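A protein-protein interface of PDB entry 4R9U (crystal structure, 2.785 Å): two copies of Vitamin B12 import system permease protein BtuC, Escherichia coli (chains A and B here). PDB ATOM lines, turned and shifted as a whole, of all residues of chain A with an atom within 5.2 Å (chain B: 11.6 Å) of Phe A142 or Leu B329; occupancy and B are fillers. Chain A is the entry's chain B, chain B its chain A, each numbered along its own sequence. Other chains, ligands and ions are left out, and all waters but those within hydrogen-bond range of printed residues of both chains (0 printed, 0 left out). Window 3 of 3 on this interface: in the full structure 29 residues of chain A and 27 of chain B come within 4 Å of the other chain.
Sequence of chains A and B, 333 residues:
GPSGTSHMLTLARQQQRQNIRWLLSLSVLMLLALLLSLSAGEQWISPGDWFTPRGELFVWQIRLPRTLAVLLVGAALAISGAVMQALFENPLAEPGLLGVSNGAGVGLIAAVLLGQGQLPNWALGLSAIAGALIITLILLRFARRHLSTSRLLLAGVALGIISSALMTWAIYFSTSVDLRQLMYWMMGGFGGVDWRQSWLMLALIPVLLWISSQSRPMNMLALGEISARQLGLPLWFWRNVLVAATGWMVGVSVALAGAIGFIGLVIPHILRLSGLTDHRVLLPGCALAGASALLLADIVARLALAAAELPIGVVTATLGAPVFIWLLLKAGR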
ATOM      1  N   ILE A 138     -28.899   7.734  -4.249  1.00  0.00           N
ATOM      2  CA  ILE A 138     -28.282   7.750  -2.935  1.00  0.00           C
ATOM      3  C   ILE A 138     -26.852   8.291  -2.990  1.00  0.00           C
ATOM      4  O   ILE A 138     -26.484   9.191  -2.209  1.00  0.00           O
ATOM      5  CB  ILE A 138     -28.274   6.358  -2.377  1.00  0.00           C
ATOM      6  CG1 ILE A 138     -29.705   5.907  -2.107  1.00  0.00           C
ATOM      7  CG2 ILE A 138     -27.371   6.272  -1.166  1.00  0.00           C
ATOM      8  CD1 ILE A 138     -29.767   4.454  -1.909  1.00  0.00           C
ATOM      9  N   LEU A 139     -26.066   7.731  -3.907  1.00  0.00           N
ATOM     10  CA  LEU A 139     -24.689   8.155  -4.163  1.00  0.00           C
ATOM     11  C   LEU A 139     -24.571   9.662  -4.376  1.00  0.00           C
ATOM     12  O   LEU A 139     -23.635  10.296  -3.877  1.00  0.00           O
ATOM     13  CB  LEU A 139     -24.134   7.422  -5.373  1.00  0.00           C
ATOM     14  CG  LEU A 139     -23.687   6.001  -5.021  1.00  0.00           C
ATOM     15  CD1 LEU A 139     -23.161   5.245  -6.244  1.00  0.00           C
ATOM     16  CD2 LEU A 139     -22.660   6.062  -3.885  1.00  0.00           C
ATOM     17  N   LEU A 140     -25.521  10.216  -5.135  1.00  0.00           N
ATOM     18  CA  LEU A 140     -25.582  11.662  -5.343  1.00  0.00           C
ATOM     19  C   LEU A 140     -25.799  12.379  -4.007  1.00  0.00           C
ATOM     20  O   LEU A 140     -25.118  13.366  -3.708  1.00  0.00           O
ATOM     21  CB  LEU A 140     -26.692  12.008  -6.338  1.00  0.00           C
ATOM     22  CG  LEU A 140     -26.456  11.380  -7.714  1.00  0.00           C
ATOM     23  CD1 LEU A 140     -27.303  12.025  -8.784  1.00  0.00           C
ATOM     24  CD2 LEU A 140     -24.977  11.510  -8.062  1.00  0.00           C
ATOM     25  N   ARG A 141     -26.666  11.839  -3.149  1.00  0.00           N
ATOM     26  CA  ARG A 141     -26.851  12.531  -1.876  1.00  0.00           C
ATOM     27  C   ARG A 141     -25.579  12.463  -1.052  1.00  0.00           C
ATOM     28  O   ARG A 141     -25.302  13.385  -0.287  1.00  0.00           O
ATOM     29  CB  ARG A 141     -28.001  11.942  -1.082  1.00  0.00           C
ATOM     30  CG  ARG A 141     -29.346  12.339  -1.598  1.00  0.00           C
ATOM     31  CD  ARG A 141     -30.437  11.917  -0.642  1.00  0.00           C
ATOM     32  NE  ARG A 141     -31.740  12.221  -1.221  1.00  0.00           N
ATOM     33  CZ  ARG A 141     -32.892  11.737  -0.777  1.00  0.00           C
ATOM     34  NH1 ARG A 141     -32.906  10.912   0.261  1.00  0.00           N
ATOM     35  NH2 ARG A 141     -34.031  12.073  -1.373  1.00  0.00           N
ATOM     36  N   PHE A 142     -24.749  11.448  -1.288  1.00  0.00           N
ATOM     37  CA  PHE A 142     -23.508  11.303  -0.519  1.00  0.00           C
ATOM     38  C   PHE A 142     -22.428  12.217  -1.082  1.00  0.00           C
ATOM     39  O   PHE A 142     -21.491  12.594  -0.369  1.00  0.00           O
ATOM     40  CB  PHE A 142     -22.993   9.852  -0.505  1.00  0.00           C
ATOM     41  CG  PHE A 142     -23.863   8.900   0.274  1.00  0.00           C
ATOM     42  CD1 PHE A 142     -23.437   7.603   0.569  1.00  0.00           C
ATOM     43  CD2 PHE A 142     -25.118   9.291   0.701  1.00  0.00           C
ATOM     44  CE1 PHE A 142     -24.254   6.729   1.286  1.00  0.00           C
ATOM     45  CE2 PHE A 142     -25.934   8.433   1.410  1.00  0.00           C
ATOM     46  CZ  PHE A 142     -25.502   7.145   1.702  1.00  0.00           C
ATOM     47  N   ALA A 143     -22.555  12.560  -2.358  1.00  0.00           N
ATOM     48  CA  ALA A 143     -21.564  13.403  -3.012  1.00  0.00           C
ATOM     49  C   ALA A 143     -21.840  14.886  -2.794  1.00  0.00           C
ATOM     50  O   ALA A 143     -20.924  15.663  -2.507  1.00  0.00           O
ATOM     51  CB  ALA A 143     -21.515  13.087  -4.492  1.00  0.00           C
ATOM     52  N   ARG A 144     -23.104  15.265  -2.918  1.00  0.00           N
ATOM     53  CA  ARG A 144     -23.546  16.650  -2.811  1.00  0.00           C
ATOM     54  C   ARG A 144     -23.114  17.296  -1.492  1.00  0.00           C
ATOM     55  O   ARG A 144     -22.990  18.517  -1.390  1.00  0.00           O
ATOM     56  CB  ARG A 144     -25.058  16.681  -2.979  1.00  0.00           C
ATOM     57  CG  ARG A 144     -25.463  16.245  -4.385  1.00  0.00           C
ATOM     58  CD  ARG A 144     -25.839  17.413  -5.275  1.00  0.00           C
ATOM     59  NE  ARG A 144     -27.005  18.134  -4.762  1.00  0.00           N
ATOM     60  CZ  ARG A 144     -28.194  18.181  -5.360  1.00  0.00           C
ATOM     61  NH1 ARG A 144     -29.195  18.860  -4.803  1.00  0.00           N
ATOM     62  NH2 ARG A 144     -28.386  17.553  -6.514  1.00  0.00           N
ATOM     63  N   ARG A 145     -22.841  16.455  -0.505  1.00  0.00           N
ATOM     64  CA  ARG A 145     -22.416  16.898   0.807  1.00  0.00           C
ATOM     65  C   ARG A 145     -20.965  17.412   0.831  1.00  0.00           C
ATOM     66  O   ARG A 145     -20.431  17.706   1.901  1.00  0.00           O
ATOM     67  CB  ARG A 145     -22.586  15.758   1.800  1.00  0.00           C
ATOM     68  CG  ARG A 145     -22.920  16.221   3.181  1.00  0.00           C
ATOM     69  CD  ARG A 145     -22.444  15.217   4.191  1.00  0.00           C
ATOM     70  NE  ARG A 145     -23.563  14.688   4.953  1.00  0.00           N
ATOM     71  CZ  ARG A 145     -23.435  13.842   5.965  1.00  0.00           C
ATOM     72  NH1 ARG A 145     -22.225  13.431   6.320  1.00  0.00           N
ATOM     73  NH2 ARG A 145     -24.500  13.400   6.619  1.00  0.00           N
ATOM     74  N   HIS A 146     -20.336  17.469  -0.344  1.00  0.00           N
ATOM     75  CA  HIS A 146     -18.955  17.957  -0.532  1.00  0.00           C
ATOM     76  C   HIS A 146     -17.920  16.979   0.009  1.00  0.00           C
ATOM     77  O   HIS A 146     -16.809  17.378   0.372  1.00  0.00           O
ATOM     78  CB  HIS A 146     -18.734  19.334   0.117  1.00  0.00           C
ATOM     79  CG  HIS A 146     -19.054  20.489  -0.783  1.00  0.00           C
ATOM     80  ND1 HIS A 146     -18.479  21.735  -0.636  1.00  0.00           N
ATOM     81  CD2 HIS A 146     -19.894  20.583  -1.841  1.00  0.00           C
ATOM     82  CE1 HIS A 146     -18.964  22.551  -1.554  1.00  0.00           C
ATOM     83  NE2 HIS A 146     -19.822  21.877  -2.298  1.00  0.00           N
ATOM     84  N   LEU A 147     -18.280  15.702   0.059  1.00  0.00           N
ATOM     85  CA  LEU A 147     -17.371  14.690   0.580  1.00  0.00           C
ATOM     86  C   LEU A 147     -16.145  14.594  -0.324  1.00  0.00           C
ATOM     87  O   LEU A 147     -16.267  14.707  -1.540  1.00  0.00           O
ATOM     88  CB  LEU A 147     -18.078  13.331   0.666  1.00  0.00           C
ATOM     89  CG  LEU A 147     -18.524  12.765   2.018  1.00  0.00           C
ATOM     90  CD1 LEU A 147     -19.926  13.246   2.381  1.00  0.00           C
ATOM     91  CD2 LEU A 147     -18.443  11.237   2.010  1.00  0.00           C
ATOM     92  N   LEU A 152     -16.110   9.404  -0.595  1.00  0.00           N
ATOM     93  CA  LEU A 152     -17.226   9.025  -1.474  1.00  0.00           C
ATOM     94  C   LEU A 152     -17.094   7.631  -2.065  1.00  0.00           C
ATOM     95  O   LEU A 152     -18.070   6.894  -2.169  1.00  0.00           O
ATOM     96  CB  LEU A 152     -17.368  10.033  -2.611  1.00  0.00           C
ATOM     97  CG  LEU A 152     -18.650   9.966  -3.446  1.00  0.00           C
ATOM     98  CD1 LEU A 152     -18.737   8.860  -4.463  1.00  0.00           C
ATOM     99  CD2 LEU A 152     -19.814   9.887  -2.512  1.00  0.00           C
ATOM    100  N   ALA A 155     -17.662   5.052   0.801  1.00  0.00           N
ATOM    101  CA  ALA A 155     -19.082   4.937   1.060  1.00  0.00           C
ATOM    102  C   ALA A 155     -19.782   4.152  -0.053  1.00  0.00           C
ATOM    103  O   ALA A 155     -20.568   3.244   0.230  1.00  0.00           O
ATOM    104  CB  ALA A 155     -19.697   6.311   1.208  1.00  0.00           C
ATOM    105  N   LEU A 159     -22.060   0.757   0.079  1.00  0.00           N
ATOM    106  CA  LEU A 159     -23.384   0.519  -0.521  1.00  0.00           C
ATOM    107  C   LEU A 159     -23.391  -0.787  -1.303  1.00  0.00           C
ATOM    108  O   LEU A 159     -24.355  -1.544  -1.242  1.00  0.00           O
ATOM    109  CB  LEU A 159     -23.797   1.640  -1.468  1.00  0.00           C
ATOM    110  CG  LEU A 159     -24.683   2.760  -0.959  1.00  0.00           C
ATOM    111  CD1 LEU A 159     -25.333   3.482  -2.120  1.00  0.00           C
ATOM    112  CD2 LEU A 159     -25.726   2.138  -0.099  1.00  0.00           C
ATOM    113  N   ILE B 270     -12.138   1.260   9.088  1.00  0.00           N
ATOM    114  CA  ILE B 270     -12.864   1.731  10.258  1.00  0.00           C
ATOM    115  C   ILE B 270     -11.925   2.261  11.325  1.00  0.00           C
ATOM    116  O   ILE B 270     -12.190   3.281  11.943  1.00  0.00           O
ATOM    117  CB  ILE B 270     -13.727   0.620  10.868  1.00  0.00           C
ATOM    118  CG1 ILE B 270     -14.916   0.334   9.960  1.00  0.00           C
ATOM    119  CG2 ILE B 270     -14.234   1.034  12.219  1.00  0.00           C
ATOM    120  CD1 ILE B 270     -15.748  -0.804  10.429  1.00  0.00           C
ATOM    121  N   LEU B 273     -10.481   5.603  10.242  1.00  0.00           N
ATOM    122  CA  LEU B 273     -11.517   6.635  10.298  1.00  0.00           C
ATOM    123  C   LEU B 273     -11.785   7.078  11.741  1.00  0.00           C
ATOM    124  O   LEU B 273     -12.392   8.119  11.981  1.00  0.00           O
ATOM    125  CB  LEU B 273     -12.804   6.139   9.627  1.00  0.00           C
ATOM    126  CG  LEU B 273     -12.710   6.037   8.095  1.00  0.00           C
ATOM    127  CD1 LEU B 273     -13.938   5.341   7.551  1.00  0.00           C
ATOM    128  CD2 LEU B 273     -12.513   7.387   7.414  1.00  0.00           C
ATOM    129  N   GLY B 320     -21.885  -5.765   9.008  1.00  0.00           N
ATOM    130  CA  GLY B 320     -20.800  -4.813   8.941  1.00  0.00           C
ATOM    131  C   GLY B 320     -21.085  -3.570   8.125  1.00  0.00           C
ATOM    132  O   GLY B 320     -20.944  -2.448   8.636  1.00  0.00           O
ATOM    133  N   ALA B 321     -21.441  -3.752   6.860  1.00  0.00           N
ATOM    134  CA  ALA B 321     -21.734  -2.622   5.981  1.00  0.00           C
ATOM    135  C   ALA B 321     -22.808  -1.606   6.527  1.00  0.00           C
ATOM    136  O   ALA B 321     -22.588  -0.390   6.397  1.00  0.00           O
ATOM    137  CB  ALA B 321     -22.112  -3.126   4.576  1.00  0.00           C
ATOM    138  N   PRO B 322     -23.979  -2.092   7.073  1.00  0.00           N
ATOM    139  CA  PRO B 322     -24.933  -1.145   7.683  1.00  0.00           C
ATOM    140  C   PRO B 322     -24.260  -0.217   8.699  1.00  0.00           C
ATOM    141  O   PRO B 322     -24.311   1.016   8.587  1.00  0.00           O
ATOM    142  CB  PRO B 322     -25.942  -2.068   8.379  1.00  0.00           C
ATOM    143  CG  PRO B 322     -25.941  -3.274   7.518  1.00  0.00           C
ATOM    144  CD  PRO B 322     -24.489  -3.474   7.177  1.00  0.00           C
ATOM    145  N   VAL B 323     -23.584  -0.854   9.653  1.00  0.00           N
ATOM    146  CA  VAL B 323     -22.780  -0.175  10.663  1.00  0.00           C
ATOM    147  C   VAL B 323     -21.704   0.686  10.024  1.00  0.00           C
ATOM    148  O   VAL B 323     -21.389   1.768  10.520  1.00  0.00           O
ATOM    149  CB  VAL B 323     -22.057  -1.165  11.576  1.00  0.00           C
ATOM    150  CG1 VAL B 323     -21.129  -0.422  12.536  1.00  0.00           C
ATOM    151  CG2 VAL B 323     -23.039  -2.034  12.333  1.00  0.00           C
ATOM    152  N   PHE B 324     -21.112   0.187   8.937  1.00  0.00           N
ATOM    153  CA  PHE B 324     -20.063   0.916   8.212  1.00  0.00           C
ATOM    154  C   PHE B 324     -20.580   2.266   7.660  1.00  0.00           C
ATOM    155  O   PHE B 324     -19.987   3.310   7.943  1.00  0.00           O
ATOM    156  CB  PHE B 324     -19.458   0.053   7.069  1.00  0.00           C
ATOM    157  CG  PHE B 324     -18.180   0.638   6.442  1.00  0.00           C
ATOM    158  CD1 PHE B 324     -17.292   1.399   7.206  1.00  0.00           C
ATOM    159  CD2 PHE B 324     -17.836   0.360   5.107  1.00  0.00           C
ATOM    160  CE1 PHE B 324     -16.118   1.915   6.645  1.00  0.00           C
ATOM    161  CE2 PHE B 324     -16.657   0.871   4.541  1.00  0.00           C
ATOM    162  CZ  PHE B 324     -15.801   1.647   5.312  1.00  0.00           C
ATOM    163  N   ILE B 325     -21.679   2.232   6.881  1.00  0.00           N
ATOM    164  CA  ILE B 325     -22.322   3.473   6.391  1.00  0.00           C
ATOM    165  C   ILE B 325     -22.668   4.429   7.517  1.00  0.00           C
ATOM    166  O   ILE B 325     -22.594   5.651   7.377  1.00  0.00           O
ATOM    167  CB  ILE B 325     -23.654   3.207   5.635  1.00  0.00           C
ATOM    168  CG1 ILE B 325     -23.498   2.095   4.628  1.00  0.00           C
ATOM    169  CG2 ILE B 325     -24.094   4.445   4.845  1.00  0.00           C
ATOM    170  CD1 ILE B 325     -22.711   2.584   3.380  1.00  0.00           C
ATOM    171  N   TRP B 326     -23.012   3.860   8.650  1.00  0.00           N
ATOM    172  CA  TRP B 326     -23.426   4.650   9.793  1.00  0.00           C
ATOM    173  C   TRP B 326     -22.226   5.441  10.285  1.00  0.00           C
ATOM    174  O   TRP B 326     -22.393   6.455  10.959  1.00  0.00           O
ATOM    175  CB  TRP B 326     -23.969   3.739  10.885  1.00  0.00           C
ATOM    176  CG  TRP B 326     -24.310   4.416  12.173  1.00  0.00           C
ATOM    177  CD1 TRP B 326     -23.483   4.651  13.240  1.00  0.00           C
ATOM    178  CD2 TRP B 326     -25.591   4.928  12.533  1.00  0.00           C
ATOM    179  NE1 TRP B 326     -24.181   5.289  14.241  1.00  0.00           N
ATOM    180  CE2 TRP B 326     -25.479   5.470  13.829  1.00  0.00           C
ATOM    181  CE3 TRP B 326     -26.824   4.983  11.879  1.00  0.00           C
ATOM    182  CZ2 TRP B 326     -26.562   6.062  14.483  1.00  0.00           C
ATOM    183  CZ3 TRP B 326     -27.897   5.568  12.529  1.00  0.00           C
ATOM    184  CH2 TRP B 326     -27.759   6.101  13.817  1.00  0.00           C
ATOM    185  N   LEU B 327     -21.018   4.989   9.955  1.00  0.00           N
ATOM    186  CA  LEU B 327     -19.786   5.662  10.392  1.00  0.00           C
ATOM    187  C   LEU B 327     -19.242   6.690   9.394  1.00  0.00           C
ATOM    188  O   LEU B 327     -18.511   7.603   9.784  1.00  0.00           O
ATOM    189  CB  LEU B 327     -18.693   4.636  10.703  1.00  0.00           C
ATOM    190  CG  LEU B 327     -18.656   4.155  12.160  1.00  0.00           C
ATOM    191  CD1 LEU B 327     -18.240   2.695  12.242  1.00  0.00           C
ATOM    192  CD2 LEU B 327     -17.728   5.022  13.004  1.00  0.00           C
ATOM    193  N   LEU B 328     -19.540   6.513   8.107  1.00  0.00           N
ATOM    194  CA  LEU B 328     -19.144   7.500   7.095  1.00  0.00           C
ATOM    195  C   LEU B 328     -20.238   8.556   6.873  1.00  0.00           C
ATOM    196  O   LEU B 328     -19.932   9.716   6.575  1.00  0.00           O
ATOM    197  CB  LEU B 328     -18.804   6.822   5.765  1.00  0.00           C
ATOM    198  CG  LEU B 328     -18.245   5.405   5.790  1.00  0.00           C
ATOM    199  CD1 LEU B 328     -19.201   4.511   5.036  1.00  0.00           C
ATOM    200  CD2 LEU B 328     -16.869   5.367   5.165  1.00  0.00           C
ATOM    201  N   LEU B 329     -21.503   8.132   7.018  1.00  0.00           N
ATOM    202  CA  LEU B 329     -22.679   9.001   6.843  1.00  0.00           C
ATOM    203  C   LEU B 329     -22.502  10.301   7.609  1.00  0.00           C
ATOM    204  O   LEU B 329     -22.673  11.388   7.072  1.00  0.00           O
ATOM    205  CB  LEU B 329     -23.979   8.313   7.327  1.00  0.00           C
ATOM    206  CG  LEU B 329     -24.872   7.444   6.432  1.00  0.00           C
ATOM    207  CD1 LEU B 329     -26.286   7.325   6.988  1.00  0.00           C
ATOM    208  CD2 LEU B 329     -24.899   7.976   5.019  1.00  0.00           C
ATOM    209  N   LYS B 330     -22.127  10.178   8.876  1.00  0.00           N
ATOM    210  CA  LYS B 330     -21.959  11.354   9.702  1.00  0.00           C
ATOM    211  C   LYS B 330     -20.531  11.414  10.244  1.00  0.00           C
ATOM    212  O   LYS B 330     -19.740  12.262   9.823  1.00  0.00           O
ATOM    213  CB  LYS B 330     -22.990  11.339  10.845  1.00  0.00           C
ATOM    214  CG  LYS B 330     -24.406  10.836  10.460  1.00  0.00           C
ATOM    215  CD  LYS B 330     -25.155  11.813   9.540  1.00  0.00           C
ATOM    216  CE  LYS B 330     -25.819  11.115   8.343  1.00  0.00           C
ATOM    217  NZ  LYS B 330     -26.766  10.032   8.731  1.00  0.00           N
ATOM    218  N   ALA B 331     -20.201  10.495  11.148  1.00  0.00           N
ATOM    219  CA  ALA B 331     -18.875  10.444  11.761  1.00  0.00           C
ATOM    220  C   ALA B 331     -17.759  10.306  10.716  1.00  0.00           C
ATOM    221  O   ALA B 331     -17.223  11.306  10.219  1.00  0.00           O
ATOM    222  CB  ALA B 331     -18.807   9.302  12.770  1.00  0.00           C
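Ile A138 touches none of the printed residues of chain B. No residue of chain B comes within 4 Å of Ala A143. Arg A145 touches just these residues of chain B: Leu B329 and Lys B330. Leu A152 touches none of the printed residues of chain B. Of the printed residues of chain B, Ala A155 touches Ile B325. Of the printed residues of chain B, Leu A159 touches Ile B325 (3.8 Å). Of the printed residues of chain A, Ile B325 touches Ala A155 and Leu A159. Leu B329 touches just these residues of chain A: Phe A142 (3.5 Å) and Arg A145 (2.2 Å). Printed residues of chain A within 4 Å of Lys B330: Arg A145. The nearest residue of chain B that does not touch Phe A142 is Ile B325 (4.2 Å). The nearest printed residue of chain A that does not touch Leu B329 is Leu A147 (5.7 Å).
Among the printed residues, pairs that only touch across the chains: Phe A142 with Leu B329 (3.5 Å), Arg A145 with Lys B330 (3.2 Å), Ala A155 with Ile B325 (3.9 Å) and Leu A159 with Ile B325 (3.8 Å).
No position is printed for both chains. Of the 5 pairs that touch across the chains among the printed residues, none has its exchanged pair printed and touching as well.
The backbone carbonyl oxygen (O) of Leu B329 lies within hydrogen-bond range of the guanidinium group (NH2) of Arg A145 (2.8 Å).
Along chain B the printed residues that touch a printed residue of chain A span positions 325 to 330. Hydrophobic or aromatic side chains of chain A within 4 Å of the printed part of chain B: Phe A142. Along chain A the printed residues that touch a printed residue of chain B span positions 142 to 159. Among the printed residues, 5 pairs touch across the chains. Among the printed residues, no Asp or Glu carboxylate lies within 4 Å of a Lys or Arg side-chain nitrogen of the other chain.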
